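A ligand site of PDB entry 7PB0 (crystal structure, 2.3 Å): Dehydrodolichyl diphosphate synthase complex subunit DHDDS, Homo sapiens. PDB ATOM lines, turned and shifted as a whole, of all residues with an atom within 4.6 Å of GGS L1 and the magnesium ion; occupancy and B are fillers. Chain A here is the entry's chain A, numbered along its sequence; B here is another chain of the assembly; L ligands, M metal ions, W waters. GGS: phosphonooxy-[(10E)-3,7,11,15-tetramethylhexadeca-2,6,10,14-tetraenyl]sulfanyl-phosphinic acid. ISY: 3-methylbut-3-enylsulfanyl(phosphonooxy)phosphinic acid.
The backbone NH of Arg 44 lies within hydrogen-bond range of an oxygen (O3A) of GGS L1, at 3.0 Å. The side-chain amide nitrogen of Asn 89 is in hydrogen-bond range of an oxygen (O8) of ISY L2. An oxygen (O2A) of GGS L1 lies within salt-bridge range of the guanidinium group of Arg 92 (2.7 Å). The backbone NH (N) of Arg 45 is in hydrogen-bond range of an oxygen (O3B) of GGS L1, at 3.1 Å. The guanidinium group (NE) of Arg 45 lies within salt-bridge range of an oxygen (O3B) of GGS L1 (2.6 Å). O2B of GGS L1 is in salt-bridge range of NE of Arg 44 (3.0 Å). N of Asn 43 lies within hydrogen-bond range of O3A of GGS L1. A sulfur (S1) of GGS L1 lies close to the backbone NH (N) of Gly 42 (3.4 Å). An oxygen (O8) of ISY L2 lies within salt-bridge range of the guanidinium group (NH2) of Arg 92 (3.9 Å).
N of Trp 239 sits at hydrogen-bond distance from O of Asp 41. The indole nitrogen (NE1) of Trp 239 lies close to the side-chain sulfur (SD) of Met 40 (3.7 Å). A ring nitrogen (ND1) of His 58 sits at hydrogen-bond distance from the side-chain amide nitrogen (ND2) of Asn 43 (3.0 Å). O of Gly 61 sits at hydrogen-bond distance from NE1 of Trp 239 (3.0 Å). NH2 of Arg 45 is in salt-bridge range of OD2 of Asp 41 (3.4 Å).
The backbone carbonyl oxygen (O) of Met 40 sits close to a sulfur (S1) of GGS L1, 3.4 Å away. CE1 of His 58 touches O2A of GGS L1, 3.3 Å away. Gly 61 touches GGS L1 (O to C10, 3.4 Å). Phe 62 touches GGS L1 (N to C10, 3.6 Å). Leu 65 touches GGS L1 (CD2 to C14, 3.4 Å). Ala 84 touches GGS L1 (O to C5, 3.1 Å). Leu 100 touches GGS L1 (O to C20, 3.3 Å). Ala 104 touches GGS L1 (CB to C19, 3.4 Å). CG1 of Val 159 touches C14 of GGS L1, at 3.7 Å. Phe 161 touches GGS L1. Hydrophobic or aromatic side chains within 4 Å of GGS L1: His 58, Leu 65, Ala 84, Leu 100, Ala 104, Val 159 and Phe 161. 16 residues have an atom within 4 Å of GGS L1: Met 40, Asp 41, Gly 42, Asn 43, Arg 44, Arg 45, His 58, Gly 61, Phe 62, Leu 65, Ala 84, Arg 92, Leu 100, Ala 104, Val 159 and Phe 161. The nearest printed residue that does not touch GGS L1 is Asn 89 (4.01 Å).
Residues that only touch the magnesium ion: Arg 45 (3.7 Å). Within 4 Å of the magnesium ion: Asp 41 and Arg 45. The nearest printed residue that does not touch the magnesium ion is Gly 42 (4.3 Å).
O7 of ISY L2 binds the magnesium ion. An oxygen (O1B) of GGS L1 is bound to the magnesium ion (2.0 Å). The magnesium ion is bound by OD1 of Asp 41 (2.0 Å). Water W1 is bound to the magnesium ion. An oxygen (O1A) of GGS L1 binds the magnesium ion (2.2 Å). Water W2 is bound to the magnesium ion (2.5 Å). The magnesium ion has six donor atoms within binding distance.
Water W1 lies within hydrogen-bond range of OD2 of Asp 41 (2.4 Å), NH2 of Arg 216 of chain B (3.0 Å), O6 of ISY L2 (3.0 Å) and NH2 of Arg 45 (3.3 Å). Water W2 lies within hydrogen-bond range of the guanidinium group of Arg 216 of chain B, an oxygen (O2B) of GGS L1 and the guanidinium group of Arg 44.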
ATOM      1  N   MET A  40     -23.971  -7.885 -14.755  1.00  0.00           N
ATOM      2  CA  MET A  40     -24.970  -8.274 -15.739  1.00  0.00           C
ATOM      3  C   MET A  40     -25.017  -7.227 -16.859  1.00  0.00           C
ATOM      4  O   MET A  40     -25.874  -6.356 -16.910  1.00  0.00           O
ATOM      5  CB  MET A  40     -26.322  -8.435 -15.073  1.00  0.00           C
ATOM      6  CG  MET A  40     -26.290  -9.420 -13.919  1.00  0.00           C
ATOM      7  SD  MET A  40     -27.872  -9.411 -13.059  1.00  0.00           S
ATOM      8  CE  MET A  40     -27.759  -7.842 -12.202  1.00  0.00           C
ATOM      9  N   ASP A  41     -24.090  -7.365 -17.798  1.00  0.00           N
ATOM     10  CA  ASP A  41     -23.854  -6.347 -18.815  1.00  0.00           C
ATOM     11  C   ASP A  41     -24.323  -6.814 -20.185  1.00  0.00           C
ATOM     12  O   ASP A  41     -24.255  -8.002 -20.523  1.00  0.00           O
ATOM     13  CB  ASP A  41     -22.368  -5.990 -18.864  1.00  0.00           C
ATOM     14  CG  ASP A  41     -22.104  -4.751 -19.689  1.00  0.00           C
ATOM     15  OD1 ASP A  41     -23.079  -4.056 -20.032  1.00  0.00           O
ATOM     16  OD2 ASP A  41     -20.910  -4.491 -19.996  1.00  0.00           O
ATOM     17  N   GLY A  42     -24.813  -5.863 -20.982  1.00  0.00           N
ATOM     18  CA  GLY A  42     -25.173  -6.095 -22.359  1.00  0.00           C
ATOM     19  C   GLY A  42     -26.659  -6.069 -22.668  1.00  0.00           C
ATOM     20  O   GLY A  42     -27.057  -6.512 -23.759  1.00  0.00           O
ATOM     21  N   ASN A  43     -27.481  -5.555 -21.755  1.00  0.00           N
ATOM     22  CA  ASN A  43     -28.930  -5.571 -21.954  1.00  0.00           C
ATOM     23  C   ASN A  43     -29.347  -4.719 -23.141  1.00  0.00           C
ATOM     24  O   ASN A  43     -30.281  -5.067 -23.875  1.00  0.00           O
ATOM     25  CB  ASN A  43     -29.638  -5.093 -20.689  1.00  0.00           C
ATOM     26  CG  ASN A  43     -29.442  -6.033 -19.527  1.00  0.00           C
ATOM     27  OD1 ASN A  43     -28.731  -7.034 -19.629  1.00  0.00           O
ATOM     28  ND2 ASN A  43     -30.058  -5.706 -18.395  1.00  0.00           N
ATOM     29  N   ARG A  44     -28.678  -3.580 -23.339  1.00  0.00           N
ATOM     30  CA  ARG A  44     -29.126  -2.668 -24.395  1.00  0.00           C
ATOM     31  C   ARG A  44     -28.705  -3.156 -25.774  1.00  0.00           C
ATOM     32  O   ARG A  44     -29.484  -3.044 -26.726  1.00  0.00           O
ATOM     33  CB  ARG A  44     -28.591  -1.257 -24.121  1.00  0.00           C
ATOM     34  CG  ARG A  44     -29.086  -0.652 -22.799  1.00  0.00           C
ATOM     35  CD  ARG A  44     -28.692   0.838 -22.666  1.00  0.00           C
ATOM     36  NE  ARG A  44     -27.245   1.003 -22.523  1.00  0.00           N
ATOM     37  CZ  ARG A  44     -26.630   2.169 -22.373  1.00  0.00           C
ATOM     38  NH1 ARG A  44     -27.322   3.304 -22.344  1.00  0.00           N
ATOM     39  NH2 ARG A  44     -25.308   2.217 -22.253  1.00  0.00           N
ATOM     40  N   ARG A  45     -27.498  -3.708 -25.898  1.00  0.00           N
ATOM     41  CA  ARG A  45     -27.094  -4.294 -27.177  1.00  0.00           C
ATOM     42  C   ARG A  45     -28.028  -5.438 -27.560  1.00  0.00           C
ATOM     43  O   ARG A  45     -28.389  -5.601 -28.733  1.00  0.00           O
ATOM     44  CB  ARG A  45     -25.645  -4.774 -27.106  1.00  0.00           C
ATOM     45  CG  ARG A  45     -24.622  -3.660 -27.224  1.00  0.00           C
ATOM     46  CD  ARG A  45     -23.274  -4.111 -26.683  1.00  0.00           C
ATOM     47  NE  ARG A  45     -23.171  -3.942 -25.233  1.00  0.00           N
ATOM     48  CZ  ARG A  45     -22.160  -4.412 -24.499  1.00  0.00           C
ATOM     49  NH1 ARG A  45     -21.164  -5.061 -25.075  1.00  0.00           N
ATOM     50  NH2 ARG A  45     -22.151  -4.222 -23.182  1.00  0.00           N
ATOM     51  N   HIS A  58     -33.899  -4.652 -20.509  1.00  0.00           N
ATOM     52  CA  HIS A  58     -33.627  -4.732 -19.079  1.00  0.00           C
ATOM     53  C   HIS A  58     -34.580  -5.677 -18.375  1.00  0.00           C
ATOM     54  O   HIS A  58     -34.185  -6.363 -17.425  1.00  0.00           O
ATOM     55  CB  HIS A  58     -33.718  -3.345 -18.459  1.00  0.00           C
ATOM     56  CG  HIS A  58     -32.538  -2.471 -18.736  1.00  0.00           C
ATOM     57  ND1 HIS A  58     -31.233  -2.898 -18.549  1.00  0.00           N
ATOM     58  CD2 HIS A  58     -32.450  -1.190 -19.161  1.00  0.00           C
ATOM     59  CE1 HIS A  58     -30.412  -1.921 -18.861  1.00  0.00           C
ATOM     60  NE2 HIS A  58     -31.116  -0.876 -19.239  1.00  0.00           N
ATOM     61  N   GLY A  61     -33.431  -8.860 -18.853  1.00  0.00           N
ATOM     62  CA  GLY A  61     -32.300  -9.004 -17.960  1.00  0.00           C
ATOM     63  C   GLY A  61     -32.706  -9.497 -16.577  1.00  0.00           C
ATOM     64  O   GLY A  61     -31.997 -10.308 -15.974  1.00  0.00           O
ATOM     65  N   PHE A  62     -33.847  -9.024 -16.073  1.00  0.00           N
ATOM     66  CA  PHE A  62     -34.322  -9.521 -14.784  1.00  0.00           C
ATOM     67  C   PHE A  62     -34.732 -10.993 -14.874  1.00  0.00           C
ATOM     68  O   PHE A  62     -34.437 -11.777 -13.970  1.00  0.00           O
ATOM     69  CB  PHE A  62     -35.505  -8.696 -14.280  1.00  0.00           C
ATOM     70  CG  PHE A  62     -36.156  -9.285 -13.073  1.00  0.00           C
ATOM     71  CD1 PHE A  62     -35.576  -9.149 -11.817  1.00  0.00           C
ATOM     72  CD2 PHE A  62     -37.318 -10.038 -13.191  1.00  0.00           C
ATOM     73  CE1 PHE A  62     -36.159  -9.710 -10.695  1.00  0.00           C
ATOM     74  CE2 PHE A  62     -37.904 -10.608 -12.070  1.00  0.00           C
ATOM     75  CZ  PHE A  62     -37.329 -10.448 -10.827  1.00  0.00           C
ATOM     76  N   LEU A  65     -31.840 -13.082 -14.519  1.00  0.00           N
ATOM     77  CA  LEU A  65     -31.345 -13.132 -13.151  1.00  0.00           C
ATOM     78  C   LEU A  65     -32.090 -14.192 -12.340  1.00  0.00           C
ATOM     79  O   LEU A  65     -31.472 -14.975 -11.627  1.00  0.00           O
ATOM     80  CB  LEU A  65     -31.458 -11.768 -12.487  1.00  0.00           C
ATOM     81  CG  LEU A  65     -31.077 -11.698 -11.010  1.00  0.00           C
ATOM     82  CD1 LEU A  65     -29.694 -12.282 -10.783  1.00  0.00           C
ATOM     83  CD2 LEU A  65     -31.140 -10.256 -10.501  1.00  0.00           C
ATOM     84  N   VAL A  82     -24.890  -9.357  -7.264  1.00  0.00           N
ATOM     85  CA  VAL A  82     -25.157  -8.859  -8.612  1.00  0.00           C
ATOM     86  C   VAL A  82     -25.030  -7.344  -8.644  1.00  0.00           C
ATOM     87  O   VAL A  82     -25.427  -6.644  -7.705  1.00  0.00           O
ATOM     88  CB  VAL A  82     -26.555  -9.300  -9.122  1.00  0.00           C
ATOM     89  CG1 VAL A  82     -26.661 -10.823  -9.144  1.00  0.00           C
ATOM     90  CG2 VAL A  82     -27.654  -8.700  -8.281  1.00  0.00           C
ATOM     91  N   TYR A  83     -24.445  -6.831  -9.736  1.00  0.00           N
ATOM     92  CA  TYR A  83     -24.362  -5.405 -10.013  1.00  0.00           C
ATOM     93  C   TYR A  83     -25.655  -5.003 -10.724  1.00  0.00           C
ATOM     94  O   TYR A  83     -25.837  -5.292 -11.914  1.00  0.00           O
ATOM     95  CB  TYR A  83     -23.136  -5.090 -10.852  1.00  0.00           C
ATOM     96  CG  TYR A  83     -22.530  -3.720 -10.642  1.00  0.00           C
ATOM     97  CD1 TYR A  83     -21.346  -3.366 -11.274  1.00  0.00           C
ATOM     98  CD2 TYR A  83     -23.134  -2.781  -9.801  1.00  0.00           C
ATOM     99  CE1 TYR A  83     -20.769  -2.112 -11.077  1.00  0.00           C
ATOM    100  CE2 TYR A  83     -22.565  -1.527  -9.598  1.00  0.00           C
ATOM    101  CZ  TYR A  83     -21.386  -1.199 -10.248  1.00  0.00           C
ATOM    102  OH  TYR A  83     -20.812   0.045 -10.053  1.00  0.00           O
ATOM    103  N   ALA A  84     -26.564  -4.364 -10.009  1.00  0.00           N
ATOM    104  CA  ALA A  84     -27.838  -3.988 -10.603  1.00  0.00           C
ATOM    105  C   ALA A  84     -27.899  -2.523 -11.034  1.00  0.00           C
ATOM    106  O   ALA A  84     -28.640  -2.193 -11.965  1.00  0.00           O
ATOM    107  CB  ALA A  84     -29.000  -4.282  -9.647  1.00  0.00           C
ATOM    108  N   ASN A  89     -24.375   4.952 -13.512  1.00  0.00           N
ATOM    109  CA  ASN A  89     -25.532   4.823 -14.378  1.00  0.00           C
ATOM    110  C   ASN A  89     -26.523   5.967 -14.197  1.00  0.00           C
ATOM    111  O   ASN A  89     -27.384   6.172 -15.058  1.00  0.00           O
ATOM    112  CB  ASN A  89     -26.239   3.488 -14.153  1.00  0.00           C
ATOM    113  CG  ASN A  89     -25.382   2.310 -14.562  1.00  0.00           C
ATOM    114  OD1 ASN A  89     -25.472   1.226 -13.996  1.00  0.00           O
ATOM    115  ND2 ASN A  89     -24.529   2.534 -15.564  1.00  0.00           N
ATOM    116  N   ARG A  92     -27.166   8.366 -17.202  1.00  0.00           N
ATOM    117  CA  ARG A  92     -27.939   8.065 -18.393  1.00  0.00           C
ATOM    118  C   ARG A  92     -29.156   8.974 -18.466  1.00  0.00           C
ATOM    119  O   ARG A  92     -29.450   9.743 -17.556  1.00  0.00           O
ATOM    120  CB  ARG A  92     -28.357   6.589 -18.390  1.00  0.00           C
ATOM    121  CG  ARG A  92     -27.178   5.643 -18.343  1.00  0.00           C
ATOM    122  CD  ARG A  92     -27.601   4.186 -18.318  1.00  0.00           C
ATOM    123  NE  ARG A  92     -26.458   3.308 -18.524  1.00  0.00           N
ATOM    124  CZ  ARG A  92     -26.550   2.001 -18.763  1.00  0.00           C
ATOM    125  NH1 ARG A  92     -27.741   1.423 -18.807  1.00  0.00           N
ATOM    126  NH2 ARG A  92     -25.456   1.283 -18.951  1.00  0.00           N
ATOM    127  N   LEU A 100     -35.346   2.102 -15.323  1.00  0.00           N
ATOM    128  CA  LEU A 100     -34.700   1.178 -14.405  1.00  0.00           C
ATOM    129  C   LEU A 100     -35.267   1.310 -12.990  1.00  0.00           C
ATOM    130  O   LEU A 100     -35.527   0.303 -12.332  1.00  0.00           O
ATOM    131  CB  LEU A 100     -33.192   1.394 -14.410  1.00  0.00           C
ATOM    132  CG  LEU A 100     -32.475   0.865 -15.650  1.00  0.00           C
ATOM    133  CD1 LEU A 100     -31.171   1.609 -15.883  1.00  0.00           C
ATOM    134  CD2 LEU A 100     -32.243  -0.645 -15.539  1.00  0.00           C
ATOM    135  N   LEU A 103     -38.528  -0.471 -12.907  1.00  0.00           N
ATOM    136  CA  LEU A 103     -38.320  -1.913 -12.843  1.00  0.00           C
ATOM    137  C   LEU A 103     -38.000  -2.355 -11.420  1.00  0.00           C
ATOM    138  O   LEU A 103     -38.567  -3.346 -10.929  1.00  0.00           O
ATOM    139  CB  LEU A 103     -37.202  -2.327 -13.801  1.00  0.00           C
ATOM    140  CG  LEU A 103     -37.067  -3.818 -14.099  1.00  0.00           C
ATOM    141  CD1 LEU A 103     -38.349  -4.370 -14.716  1.00  0.00           C
ATOM    142  CD2 LEU A 103     -35.879  -4.056 -15.036  1.00  0.00           C
ATOM    143  N   ALA A 104     -37.119  -1.621 -10.742  1.00  0.00           N
ATOM    144  CA  ALA A 104     -36.829  -1.912  -9.343  1.00  0.00           C
ATOM    145  C   ALA A 104     -38.063  -1.755  -8.468  1.00  0.00           C
ATOM    146  O   ALA A 104     -38.260  -2.498  -7.511  1.00  0.00           O
ATOM    147  CB  ALA A 104     -35.701  -0.995  -8.848  1.00  0.00           C
ATOM    148  N   LYS A 107     -40.139  -5.138  -9.050  1.00  0.00           N
ATOM    149  CA  LYS A 107     -39.606  -6.374  -8.505  1.00  0.00           C
ATOM    150  C   LYS A 107     -39.519  -6.330  -6.980  1.00  0.00           C
ATOM    151  O   LYS A 107     -39.917  -7.290  -6.300  1.00  0.00           O
ATOM    152  CB  LYS A 107     -38.240  -6.672  -9.118  1.00  0.00           C
ATOM    153  CG  LYS A 107     -38.252  -6.687 -10.632  1.00  0.00           C
ATOM    154  CD  LYS A 107     -39.379  -7.567 -11.151  1.00  0.00           C
ATOM    155  CE  LYS A 107     -39.581  -7.422 -12.653  1.00  0.00           C
ATOM    156  NZ  LYS A 107     -40.628  -8.336 -13.175  1.00  0.00           N
ATOM    157  N   PHE A 108     -39.024  -5.225  -6.419  1.00  0.00           N
ATOM    158  CA  PHE A 108     -38.957  -5.119  -4.970  1.00  0.00           C
ATOM    159  C   PHE A 108     -40.349  -5.102  -4.347  1.00  0.00           C
ATOM    160  O   PHE A 108     -40.505  -5.542  -3.198  1.00  0.00           O
ATOM    161  CB  PHE A 108     -38.169  -3.874  -4.551  1.00  0.00           C
ATOM    162  CG  PHE A 108     -36.684  -4.110  -4.486  1.00  0.00           C
ATOM    163  CD1 PHE A 108     -36.141  -4.929  -3.510  1.00  0.00           C
ATOM    164  CD2 PHE A 108     -35.830  -3.528  -5.415  1.00  0.00           C
ATOM    165  CE1 PHE A 108     -34.774  -5.160  -3.453  1.00  0.00           C
ATOM    166  CE2 PHE A 108     -34.468  -3.755  -5.366  1.00  0.00           C
ATOM    167  CZ  PHE A 108     -33.938  -4.570  -4.391  1.00  0.00           C
ATOM    168  N   VAL A 159     -27.855  -7.466  -3.767  1.00  0.00           N
ATOM    169  CA  VAL A 159     -28.156  -6.605  -4.902  1.00  0.00           C
ATOM    170  C   VAL A 159     -27.402  -5.297  -4.714  1.00  0.00           C
ATOM    171  O   VAL A 159     -27.725  -4.506  -3.815  1.00  0.00           O
ATOM    172  CB  VAL A 159     -29.665  -6.368  -5.051  1.00  0.00           C
ATOM    173  CG1 VAL A 159     -29.949  -5.525  -6.293  1.00  0.00           C
ATOM    174  CG2 VAL A 159     -30.401  -7.681  -5.127  1.00  0.00           C
ATOM    175  N   PHE A 161     -27.007  -1.829  -5.539  1.00  0.00           N
ATOM    176  CA  PHE A 161     -27.927  -0.858  -6.091  1.00  0.00           C
ATOM    177  C   PHE A 161     -27.411   0.534  -5.736  1.00  0.00           C
ATOM    178  O   PHE A 161     -27.242   0.849  -4.553  1.00  0.00           O
ATOM    179  CB  PHE A 161     -29.334  -1.099  -5.533  1.00  0.00           C
ATOM    180  CG  PHE A 161     -30.426  -0.372  -6.265  1.00  0.00           C
ATOM    181  CD1 PHE A 161     -31.644  -0.150  -5.655  1.00  0.00           C
ATOM    182  CD2 PHE A 161     -30.257   0.060  -7.564  1.00  0.00           C
ATOM    183  CE1 PHE A 161     -32.678   0.507  -6.327  1.00  0.00           C
ATOM    184  CE2 PHE A 161     -31.280   0.725  -8.240  1.00  0.00           C
ATOM    185  CZ  PHE A 161     -32.492   0.943  -7.622  1.00  0.00           C
ATOM    186  N   TRP A 239     -25.989 -10.476 -21.476  1.00  0.00           N
ATOM    187  CA  TRP A 239     -26.582 -10.991 -20.241  1.00  0.00           C
ATOM    188  C   TRP A 239     -27.961 -11.591 -20.433  1.00  0.00           C
ATOM    189  O   TRP A 239     -28.209 -12.694 -19.909  1.00  0.00           O
ATOM    190  CB  TRP A 239     -26.609  -9.899 -19.159  1.00  0.00           C
ATOM    191  CG  TRP A 239     -27.401 -10.349 -17.955  1.00  0.00           C
ATOM    192  CD1 TRP A 239     -28.620  -9.887 -17.555  1.00  0.00           C
ATOM    193  CD2 TRP A 239     -27.033 -11.382 -17.032  1.00  0.00           C
ATOM    194  NE1 TRP A 239     -29.024 -10.557 -16.418  1.00  0.00           N
ATOM    195  CE2 TRP A 239     -28.077 -11.476 -16.079  1.00  0.00           C
ATOM    196  CE3 TRP A 239     -25.925 -12.227 -16.899  1.00  0.00           C
ATOM    197  CZ2 TRP A 239     -28.035 -12.384 -15.016  1.00  0.00           C
ATOM    198  CZ3 TRP A 239     -25.886 -13.122 -15.842  1.00  0.00           C
ATOM    199  CH2 TRP A 239     -26.934 -13.199 -14.917  1.00  0.00           C
ATOM    200  N   ARG B 216     -17.754   3.361 -22.020  1.00  0.00           N
ATOM    201  CA  ARG B 216     -18.942   4.200 -21.988  1.00  0.00           C
ATOM    202  C   ARG B 216     -19.135   4.925 -20.657  1.00  0.00           C
ATOM    203  O   ARG B 216     -19.973   5.821 -20.585  1.00  0.00           O
ATOM    204  CB  ARG B 216     -20.176   3.359 -22.319  1.00  0.00           C
ATOM    205  CG  ARG B 216     -20.143   2.793 -23.734  1.00  0.00           C
ATOM    206  CD  ARG B 216     -21.249   1.761 -23.985  1.00  0.00           C
ATOM    207  NE  ARG B 216     -20.902   0.426 -23.518  1.00  0.00           N
ATOM    208  CZ  ARG B 216     -20.118  -0.430 -24.183  1.00  0.00           C
ATOM    209  NH1 ARG B 216     -19.588  -0.077 -25.349  1.00  0.00           N
ATOM    210  NH2 ARG B 216     -19.859  -1.628 -23.679  1.00  0.00           N
HETATM  211  C1  GGS L   1     -26.194  -3.095 -17.400  1.00  0.00           C
HETATM  212  S1  GGS L   1     -26.631  -3.739 -19.010  1.00  0.00           S
HETATM  213  C2  GGS L   1     -27.031  -3.770 -16.341  1.00  0.00           C
HETATM  214  C3  GGS L   1     -27.778  -3.101 -15.532  1.00  0.00           C
HETATM  215  C4  GGS L   1     -27.830  -1.584 -15.621  1.00  0.00           C
HETATM  216  C5  GGS L   1     -28.568  -3.879 -14.507  1.00  0.00           C
HETATM  217  C6  GGS L   1     -29.936  -4.261 -15.039  1.00  0.00           C
HETATM  218  C7  GGS L   1     -30.158  -5.735 -14.788  1.00  0.00           C
HETATM  219  C8  GGS L   1     -31.199  -6.153 -14.100  1.00  0.00           C
HETATM  220  C9  GGS L   1     -32.184  -5.147 -13.521  1.00  0.00           C
HETATM  221  PA  GGS L   1     -26.362  -2.042 -20.204  1.00  0.00           P
HETATM  222  PB  GGS L   1     -25.147  -2.316 -22.716  1.00  0.00           P
HETATM  223  C10 GGS L   1     -31.390  -7.640 -13.888  1.00  0.00           C
HETATM  224  C11 GGS L   1     -33.061  -5.823 -12.449  1.00  0.00           C
HETATM  225  C12 GGS L   1     -32.165  -6.475 -11.404  1.00  0.00           C
HETATM  226  C13 GGS L   1     -32.545  -6.568 -10.162  1.00  0.00           C
HETATM  227  C14 GGS L   1     -31.647  -7.218  -9.131  1.00  0.00           C
HETATM  228  C15 GGS L   1     -33.888  -6.010  -9.730  1.00  0.00           C
HETATM  229  C16 GGS L   1     -33.663  -4.563  -9.324  1.00  0.00           C
HETATM  230  C17 GGS L   1     -33.546  -3.720 -10.582  1.00  0.00           C
HETATM  231  C18 GGS L   1     -33.007  -2.528 -10.509  1.00  0.00           C
HETATM  232  C19 GGS L   1     -32.502  -1.969  -9.179  1.00  0.00           C
HETATM  233  O1A GGS L   1     -25.063  -1.419 -19.887  1.00  0.00           O
HETATM  234  O1B GGS L   1     -23.901  -2.484 -21.934  1.00  0.00           O
HETATM  235  C20 GGS L   1     -32.897  -1.691 -11.777  1.00  0.00           C
HETATM  236  O2A GGS L   1     -27.439  -1.075 -19.895  1.00  0.00           O
HETATM  237  O2B GGS L   1     -25.205  -0.984 -23.352  1.00  0.00           O
HETATM  238  O3A GGS L   1     -26.418  -2.453 -21.740  1.00  0.00           O
HETATM  239  O3B GGS L   1     -25.271  -3.312 -23.787  1.00  0.00           O
HETATM  240  P1  ISY L   2     -19.287   0.605 -18.592  1.00  0.00           P
HETATM  241  O2  ISY L   2     -20.012  -0.450 -17.552  1.00  0.00           O
HETATM  242  P3  ISY L   2     -21.640  -0.761 -17.466  1.00  0.00           P
HETATM  243  O4  ISY L   2     -17.985   1.055 -17.976  1.00  0.00           O
HETATM  244  O5  ISY L   2     -20.200   1.799 -18.810  1.00  0.00           O
HETATM  245  O6  ISY L   2     -19.039  -0.050 -19.932  1.00  0.00           O
HETATM  246  O7  ISY L   2     -22.217  -0.991 -18.849  1.00  0.00           O
HETATM  247  O8  ISY L   2     -22.331   0.376 -16.755  1.00  0.00           O
HETATM  248  S9  ISY L   2     -21.931  -2.551 -16.367  1.00  0.00           S
HETATM  249  C10 ISY L   2     -21.882  -2.226 -14.582  1.00  0.00           C
HETATM  250  C11 ISY L   2     -23.150  -1.503 -14.137  1.00  0.00           C
HETATM  251  C12 ISY L   2     -24.255  -2.506 -13.796  1.00  0.00           C
HETATM  252  C13 ISY L   2     -24.138  -3.984 -14.191  1.00  0.00           C
HETATM  253  C14 ISY L   2     -25.330  -2.089 -13.156  1.00  0.00           C
HETATM  254 MG    MG M   1     -22.979  -2.094 -20.254  1.00  0.00          MG
HETATM  255  O   HOH W   1     -20.905  -2.248 -20.905  1.00  0.00           O
HETATM  256  O   HOH W   2     -22.950   0.157 -21.302  1.00  0.00           O
